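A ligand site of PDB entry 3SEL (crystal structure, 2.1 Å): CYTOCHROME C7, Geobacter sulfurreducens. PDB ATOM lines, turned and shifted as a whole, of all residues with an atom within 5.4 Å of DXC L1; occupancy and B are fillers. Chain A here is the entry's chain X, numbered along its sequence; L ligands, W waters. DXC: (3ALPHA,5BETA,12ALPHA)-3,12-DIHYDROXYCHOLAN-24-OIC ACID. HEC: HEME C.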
ATOM      1  N   ILE A   4       4.593  -0.348  33.919  1.00  0.00           N
ATOM      2  CA  ILE A   4       3.657  -1.242  33.250  1.00  0.00           C
ATOM      3  C   ILE A   4       4.405  -2.167  32.314  1.00  0.00           C
ATOM      4  O   ILE A   4       5.484  -1.837  31.841  1.00  0.00           O
ATOM      5  CB  ILE A   4       2.676  -0.401  32.386  1.00  0.00           C
ATOM      6  CG1 ILE A   4       1.704   0.356  33.268  1.00  0.00           C
ATOM      7  CG2 ILE A   4       1.877  -1.275  31.367  1.00  0.00           C
ATOM      8  CD1 ILE A   4       0.848   1.262  32.501  1.00  0.00           C
ATOM      9  N   LEU A   6       3.507  -4.459  28.878  1.00  0.00           N
ATOM     10  CA  LEU A   6       2.538  -4.758  27.835  1.00  0.00           C
ATOM     11  C   LEU A   6       2.705  -6.259  27.515  1.00  0.00           C
ATOM     12  O   LEU A   6       3.812  -6.740  27.288  1.00  0.00           O
ATOM     13  CB  LEU A   6       2.811  -3.884  26.603  1.00  0.00           C
ATOM     14  CG  LEU A   6       2.825  -2.381  26.951  1.00  0.00           C
ATOM     15  CD1 LEU A   6       4.207  -1.791  27.207  1.00  0.00           C
ATOM     16  CD2 LEU A   6       2.145  -1.615  25.862  1.00  0.00           C
ATOM     17  N   PHE A  15       7.796  -0.965  30.231  1.00  0.00           N
ATOM     18  CA  PHE A  15       7.825   0.472  30.072  1.00  0.00           C
ATOM     19  C   PHE A  15       8.318   1.098  31.395  1.00  0.00           C
ATOM     20  O   PHE A  15       7.565   1.225  32.335  1.00  0.00           O
ATOM     21  CB  PHE A  15       6.450   1.010  29.701  1.00  0.00           C
ATOM     22  CG  PHE A  15       6.445   2.495  29.544  1.00  0.00           C
ATOM     23  CD1 PHE A  15       7.048   3.071  28.434  1.00  0.00           C
ATOM     24  CD2 PHE A  15       5.988   3.300  30.567  1.00  0.00           C
ATOM     25  CE1 PHE A  15       7.122   4.433  28.303  1.00  0.00           C
ATOM     26  CE2 PHE A  15       6.063   4.691  30.448  1.00  0.00           C
ATOM     27  CZ  PHE A  15       6.621   5.253  29.319  1.00  0.00           C
ATOM     28  N   LYS A  29       4.953  15.066  24.970  1.00  0.00           N
ATOM     29  CA  LYS A  29       5.130  13.966  23.998  1.00  0.00           C
ATOM     30  C   LYS A  29       4.211  12.810  24.366  1.00  0.00           C
ATOM     31  O   LYS A  29       3.753  12.104  23.521  1.00  0.00           O
ATOM     32  CB  LYS A  29       6.589  13.495  23.956  1.00  0.00           C
ATOM     33  CG  LYS A  29       7.527  14.471  23.294  1.00  0.00           C
ATOM     34  CD  LYS A  29       7.452  14.325  21.760  1.00  0.00           C
ATOM     35  CE  LYS A  29       8.026  15.534  21.027  1.00  0.00           C
ATOM     36  N   CYS A  30       3.912  12.637  25.640  1.00  0.00           N
ATOM     37  CA  CYS A  30       3.015  11.552  26.040  1.00  0.00           C
ATOM     38  C   CYS A  30       1.753  11.936  26.775  1.00  0.00           C
ATOM     39  O   CYS A  30       0.739  11.243  26.658  1.00  0.00           O
ATOM     40  CB  CYS A  30       3.793  10.550  26.890  1.00  0.00           C
ATOM     41  SG  CYS A  30       5.168   9.757  25.990  1.00  0.00           S
ATOM     42  N   LYS A  33      -2.525  14.234  25.909  1.00  0.00           N
ATOM     43  CA  LYS A  33      -2.899  13.933  24.546  1.00  0.00           C
ATOM     44  C   LYS A  33      -4.410  13.888  24.582  1.00  0.00           C
ATOM     45  O   LYS A  33      -5.037  13.696  25.619  1.00  0.00           O
ATOM     46  CB  LYS A  33      -2.261  12.650  24.078  1.00  0.00           C
ATOM     47  CG  LYS A  33      -0.769  12.775  23.917  1.00  0.00           C
ATOM     48  CD  LYS A  33      -0.460  13.338  22.578  1.00  0.00           C
ATOM     49  CE  LYS A  33       0.997  13.669  22.478  1.00  0.00           C
ATOM     50  NZ  LYS A  33       1.318  13.903  21.073  1.00  0.00           N
ATOM     51  N   LYS A  37      -6.334   7.935  23.311  1.00  0.00           N
ATOM     52  CA  LYS A  37      -4.970   7.416  23.260  1.00  0.00           C
ATOM     53  C   LYS A  37      -4.821   6.103  24.010  1.00  0.00           C
ATOM     54  O   LYS A  37      -3.936   5.364  23.701  1.00  0.00           O
ATOM     55  CB  LYS A  37      -3.951   8.413  23.798  1.00  0.00           C
ATOM     56  CG  LYS A  37      -3.581   9.571  22.845  1.00  0.00           C
ATOM     57  CD  LYS A  37      -3.028   9.122  21.494  1.00  0.00           C
ATOM     58  CE  LYS A  37      -2.398  10.288  20.760  1.00  0.00           C
ATOM     59  NZ  LYS A  37      -1.577   9.872  19.550  1.00  0.00           N
ATOM     60  N   ILE A  38      -5.674   5.841  24.988  1.00  0.00           N
ATOM     61  CA  ILE A  38      -5.701   4.546  25.680  1.00  0.00           C
ATOM     62  C   ILE A  38      -6.250   3.470  24.744  1.00  0.00           C
ATOM     63  O   ILE A  38      -5.655   2.388  24.603  1.00  0.00           O
ATOM     64  CB  ILE A  38      -6.508   4.675  26.975  1.00  0.00           C
ATOM     65  CG1 ILE A  38      -5.808   5.642  27.929  1.00  0.00           C
ATOM     66  CG2 ILE A  38      -6.674   3.300  27.690  1.00  0.00           C
ATOM     67  CD1 ILE A  38      -6.466   5.777  29.270  1.00  0.00           C
ATOM     68  N   GLU A  39      -7.361   3.773  24.074  1.00  0.00           N
ATOM     69  CA  GLU A  39      -7.938   2.834  23.116  1.00  0.00           C
ATOM     70  C   GLU A  39      -7.085   2.707  21.859  1.00  0.00           C
ATOM     71  O   GLU A  39      -7.136   1.696  21.189  1.00  0.00           O
ATOM     72  CB  GLU A  39      -9.360   3.252  22.741  1.00  0.00           C
ATOM     73  CG  GLU A  39     -10.340   3.293  23.894  1.00  0.00           C
ATOM     74  CD  GLU A  39     -11.633   4.009  23.547  1.00  0.00           C
ATOM     75  OE1 GLU A  39     -11.785   5.227  23.807  1.00  0.00           O
ATOM     76  OE2 GLU A  39     -12.514   3.338  22.996  1.00  0.00           O
ATOM     77  N   PHE A  41      -3.744   2.599  21.353  1.00  0.00           N
ATOM     78  CA  PHE A  41      -2.433   1.979  21.383  1.00  0.00           C
ATOM     79  C   PHE A  41      -2.543   0.524  20.985  1.00  0.00           C
ATOM     80  O   PHE A  41      -3.502  -0.148  21.307  1.00  0.00           O
ATOM     81  CB  PHE A  41      -1.775   2.100  22.750  1.00  0.00           C
ATOM     82  CG  PHE A  41      -0.306   1.740  22.727  1.00  0.00           C
ATOM     83  CD1 PHE A  41       0.637   2.689  22.377  1.00  0.00           C
ATOM     84  CD2 PHE A  41       0.106   0.457  22.992  1.00  0.00           C
ATOM     85  CE1 PHE A  41       1.990   2.365  22.334  1.00  0.00           C
ATOM     86  CE2 PHE A  41       1.467   0.127  22.965  1.00  0.00           C
ATOM     87  CZ  PHE A  41       2.388   1.084  22.630  1.00  0.00           C
ATOM     88  N   GLY A  42      -1.542   0.074  20.270  1.00  0.00           N
ATOM     89  CA  GLY A  42      -1.497  -1.276  19.753  1.00  0.00           C
ATOM     90  C   GLY A  42      -0.164  -1.511  19.106  1.00  0.00           C
ATOM     91  O   GLY A  42       0.783  -0.751  19.300  1.00  0.00           O
ATOM     92  N   LYS A  49       5.355   5.455  16.065  1.00  0.00           N
ATOM     93  CA  LYS A  49       5.730   6.601  16.916  1.00  0.00           C
ATOM     94  C   LYS A  49       5.435   6.363  18.402  1.00  0.00           C
ATOM     95  O   LYS A  49       6.014   7.015  19.257  1.00  0.00           O
ATOM     96  CB  LYS A  49       5.071   7.911  16.417  1.00  0.00           C
ATOM     97  CG  LYS A  49       3.567   7.979  16.692  1.00  0.00           C
ATOM     98  N   GLY A  50       4.551   5.414  18.721  1.00  0.00           N
ATOM     99  CA  GLY A  50       4.246   5.032  20.100  1.00  0.00           C
ATOM    100  C   GLY A  50       5.405   4.506  20.950  1.00  0.00           C
ATOM    101  O   GLY A  50       5.445   4.742  22.131  1.00  0.00           O
HETATM  102  C1  DXC L   1      -2.154   0.587  26.583  1.00  0.00           C
HETATM  103  C2  DXC L   1      -0.660   0.865  26.633  1.00  0.00           C
HETATM  104  C3  DXC L   1      -0.318   1.831  27.809  1.00  0.00           C
HETATM  105  C4  DXC L   1      -1.057   3.185  27.684  1.00  0.00           C
HETATM  106  C5  DXC L   1      -2.561   2.938  27.496  1.00  0.00           C
HETATM  107  C6  DXC L   1      -2.876   1.925  26.371  1.00  0.00           C
HETATM  108  C7  DXC L   1       1.214   1.998  27.924  1.00  0.00           C
HETATM  109  C8  DXC L   1       1.836   2.845  26.813  1.00  0.00           C
HETATM  110  C9  DXC L   1       1.061   4.201  26.684  1.00  0.00           C
HETATM  111  C10 DXC L   1      -0.461   4.001  26.550  1.00  0.00           C
HETATM  112  C11 DXC L   1       1.512   4.976  25.425  1.00  0.00           C
HETATM  113  C12 DXC L   1       0.887   6.392  25.353  1.00  0.00           C
HETATM  114  C13 DXC L   1      -0.628   6.245  25.215  1.00  0.00           C
HETATM  115  C14 DXC L   1      -1.200   5.371  26.335  1.00  0.00           C
HETATM  116  C15 DXC L   1       3.015   5.259  25.328  1.00  0.00           C
HETATM  117  C16 DXC L   1       3.091   6.446  24.359  1.00  0.00           C
HETATM  118  C17 DXC L   1       1.616   6.913  24.117  1.00  0.00           C
HETATM  119  C18 DXC L   1      -0.964   3.963  28.991  1.00  0.00           C
HETATM  120  C19 DXC L   1       1.617   8.427  23.874  1.00  0.00           C
HETATM  121  O1  DXC L   1      -0.958   5.644  23.975  1.00  0.00           O
HETATM  122  O2  DXC L   1      -2.510  -0.333  25.544  1.00  0.00           O
HETATM  123  C20 DXC L   1       1.255   7.162  26.611  1.00  0.00           C
HETATM  124  C21 DXC L   1       2.710   8.816  22.863  1.00  0.00           C
HETATM  125  C22 DXC L   1       2.501   8.176  21.508  1.00  0.00           C
HETATM  126  C23 DXC L   1       1.552   8.988  20.627  1.00  0.00           C
HETATM  127  O3  DXC L   1       1.919  10.064  20.135  1.00  0.00           O
HETATM  128  O4  DXC L   1       0.410   8.574  20.420  1.00  0.00           O
HETATM  129  C24 DXC L   1       0.265   9.044  23.441  1.00  0.00           C
HETATM  130 FE   HEC L   2      11.246   4.623  25.362  1.00  0.00          FE
HETATM  131  CHA HEC L   2      14.306   4.405  26.740  1.00  0.00           C
HETATM  132  CHB HEC L   2      10.658   1.303  26.145  1.00  0.00           C
HETATM  133  CHC HEC L   2       8.049   4.914  24.218  1.00  0.00           C
HETATM  134  CHD HEC L   2      11.865   7.843  24.300  1.00  0.00           C
HETATM  135  NA  HEC L   2      12.287   3.107  26.261  1.00  0.00           N
HETATM  136  C1A HEC L   2      13.507   3.268  26.813  1.00  0.00           C
HETATM  137  C2A HEC L   2      13.851   2.024  27.444  1.00  0.00           C
HETATM  138  C3A HEC L   2      12.859   1.167  27.291  1.00  0.00           C
HETATM  139  C4A HEC L   2      11.845   1.836  26.538  1.00  0.00           C
HETATM  140  CMA HEC L   2      12.802  -0.279  27.835  1.00  0.00           C
HETATM  141  CAA HEC L   2      15.184   1.717  28.154  1.00  0.00           C
HETATM  142  CBA HEC L   2      15.269   2.430  29.485  1.00  0.00           C
HETATM  143  CGA HEC L   2      16.658   2.249  30.052  1.00  0.00           C
HETATM  144  O1A HEC L   2      17.623   2.003  29.277  1.00  0.00           O
HETATM  145  O2A HEC L   2      16.800   2.359  31.295  1.00  0.00           O
HETATM  146  NB  HEC L   2       9.700   3.355  25.195  1.00  0.00           N
HETATM  147  C1B HEC L   2       9.646   2.029  25.561  1.00  0.00           C
HETATM  148  C2B HEC L   2       8.349   1.505  25.277  1.00  0.00           C
HETATM  149  C3B HEC L   2       7.614   2.495  24.774  1.00  0.00           C
HETATM  150  C4B HEC L   2       8.438   3.682  24.710  1.00  0.00           C
HETATM  151  CMB HEC L   2       7.950   0.023  25.548  1.00  0.00           C
HETATM  152  CAB HEC L   2       6.143   2.398  24.332  1.00  0.00           C
HETATM  153  CBB HEC L   2       5.273   1.863  25.236  1.00  0.00           C
HETATM  154  NC  HEC L   2      10.166   6.124  24.390  1.00  0.00           N
HETATM  155  C1C HEC L   2       8.845   6.023  24.051  1.00  0.00           C
HETATM  156  C2C HEC L   2       8.415   7.295  23.489  1.00  0.00           C
HETATM  157  C3C HEC L   2       9.471   8.117  23.532  1.00  0.00           C
HETATM  158  C4C HEC L   2      10.599   7.372  24.085  1.00  0.00           C
HETATM  159  CMC HEC L   2       6.963   7.576  22.985  1.00  0.00           C
HETATM  160  CAC HEC L   2       9.547   9.597  23.102  1.00  0.00           C
HETATM  161  CBC HEC L   2       8.428  10.370  23.112  1.00  0.00           C
HETATM  162  ND  HEC L   2      12.804   5.929  25.514  1.00  0.00           N
HETATM  163  C1D HEC L   2      12.891   7.185  24.920  1.00  0.00           C
HETATM  164  C2D HEC L   2      14.235   7.687  25.061  1.00  0.00           C
HETATM  165  C3D HEC L   2      14.991   6.618  25.809  1.00  0.00           C
HETATM  166  C4D HEC L   2      14.023   5.575  26.082  1.00  0.00           C
HETATM  167  CMD HEC L   2      14.834   9.004  24.542  1.00  0.00           C
HETATM  168  CAD HEC L   2      16.473   6.633  26.233  1.00  0.00           C
HETATM  169  CBD HEC L   2      16.484   6.662  27.749  1.00  0.00           C
HETATM  170  CGD HEC L   2      17.711   6.004  28.349  1.00  0.00           C
HETATM  171  O1D HEC L   2      18.379   5.138  27.698  1.00  0.00           O
HETATM  172  O2D HEC L   2      18.000   6.364  29.529  1.00  0.00           O
HETATM  173 FE   HEC L   3       4.588  10.121  32.511  1.00  0.00          FE
HETATM  174  CHA HEC L   3       2.803   8.030  34.560  1.00  0.00           C
HETATM  175  CHB HEC L   3       4.300  12.598  34.770  1.00  0.00           C
HETATM  176  CHC HEC L   3       6.927  11.966  30.793  1.00  0.00           C
HETATM  177  CHD HEC L   3       4.189   8.073  29.889  1.00  0.00           C
HETATM  178  NA  HEC L   3       3.665  10.280  34.265  1.00  0.00           N
HETATM  179  C1A HEC L   3       3.099   9.280  35.014  1.00  0.00           C
HETATM  180  C2A HEC L   3       2.881   9.790  36.352  1.00  0.00           C
HETATM  181  C3A HEC L   3       3.279  11.053  36.409  1.00  0.00           C
HETATM  182  C4A HEC L   3       3.779  11.381  35.098  1.00  0.00           C
HETATM  183  CMA HEC L   3       3.235  12.016  37.638  1.00  0.00           C
HETATM  184  CAA HEC L   3       2.312   8.992  37.528  1.00  0.00           C
HETATM  185  CBA HEC L   3       3.496   8.309  38.248  1.00  0.00           C
HETATM  186  CGA HEC L   3       4.816   9.085  38.219  1.00  0.00           C
HETATM  187  O1A HEC L   3       5.193   9.734  37.197  1.00  0.00           O
HETATM  188  O2A HEC L   3       5.576   9.078  39.225  1.00  0.00           O
HETATM  189  NB  HEC L   3       5.516  11.929  32.750  1.00  0.00           N
HETATM  190  C1B HEC L   3       5.215  12.811  33.762  1.00  0.00           C
HETATM  191  C2B HEC L   3       5.995  14.015  33.548  1.00  0.00           C
HETATM  192  C3B HEC L   3       6.730  13.823  32.444  1.00  0.00           C
HETATM  193  C4B HEC L   3       6.444  12.523  31.938  1.00  0.00           C
HETATM  194  CMB HEC L   3       5.966  15.240  34.485  1.00  0.00           C
HETATM  195  CAB HEC L   3       7.768  14.765  31.788  1.00  0.00           C
HETATM  196  CBB HEC L   3       8.754  15.229  32.581  1.00  0.00           C
HETATM  197  NC  HEC L   3       5.364  10.051  30.715  1.00  0.00           N
HETATM  198  C1C HEC L   3       6.345  10.879  30.184  1.00  0.00           C
HETATM  199  C2C HEC L   3       6.684  10.393  28.866  1.00  0.00           C
HETATM  200  C3C HEC L   3       5.949   9.317  28.606  1.00  0.00           C
HETATM  201  C4C HEC L   3       5.102   9.084  29.763  1.00  0.00           C
HETATM  202  CMC HEC L   3       7.732  11.118  27.977  1.00  0.00           C
HETATM  203  CAC HEC L   3       5.953   8.448  27.318  1.00  0.00           C
HETATM  204  CBC HEC L   3       7.143   8.078  26.747  1.00  0.00           C
HETATM  205  ND  HEC L   3       3.609   8.365  32.260  1.00  0.00           N
HETATM  206  C1D HEC L   3       3.612   7.696  31.061  1.00  0.00           C
HETATM  207  C2D HEC L   3       2.905   6.468  31.252  1.00  0.00           C
HETATM  208  C3D HEC L   3       2.447   6.445  32.698  1.00  0.00           C
HETATM  209  C4D HEC L   3       2.969   7.652  33.258  1.00  0.00           C
HETATM  210  CMD HEC L   3       2.615   5.422  30.195  1.00  0.00           C
HETATM  211  CAD HEC L   3       1.684   5.308  33.416  1.00  0.00           C
HETATM  212  CBD HEC L   3       2.607   4.057  33.442  1.00  0.00           C
HETATM  213  CGD HEC L   3       3.816   4.176  34.343  1.00  0.00           C
HETATM  214  O1D HEC L   3       3.733   4.829  35.408  1.00  0.00           O
HETATM  215  O2D HEC L   3       4.893   3.601  34.018  1.00  0.00           O
HETATM  216  O   HOH W   1      -1.687  -2.764  25.262  1.00  0.00           O
HETATM  217  O   HOH W   2      -0.391   6.000  21.193  1.00  0.00           O
HETATM  218  O   HOH W   3      -4.627   0.004  23.899  1.00  0.00           O
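Water W3 lies within hydrogen-bond range of O of Ile 38 (2.7 Å), O2 of DXC L1 (2.7 Å) and O of Phe 41 (2.8 Å).
Leu 6 touches DXC L1. Lys 29 touches DXC L1. Cys 30 touches DXC L1 (O to C24, 3.9 Å). Ile 38 touches DXC L1. Phe 41 touches DXC L1. O of Gly 50 touches C16 of DXC L1, at 3.7 Å. Eight residues have an atom within 4 Å of DXC L1: Leu 6, Lys 29, Cys 30, Lys 33, Lys 37, Ile 38, Phe 41 and Gly 50. The nearest printed residue that does not touch DXC L1 is Lys 49 (4.3 Å).
O of Lys 37 lies within hydrogen-bond range of O1 of DXC L1, 3.0 Å away. NZ of Lys 37 is in salt-bridge range of O4 of DXC L1, 2.5 Å away. SG of Cys 30 is bonded to CAC of HEC L3 (2.0 Å). The side-chain amino group (NZ) of Lys 33 lies within salt-bridge range of an oxygen (O3) of DXC L1 (3.997 Å).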
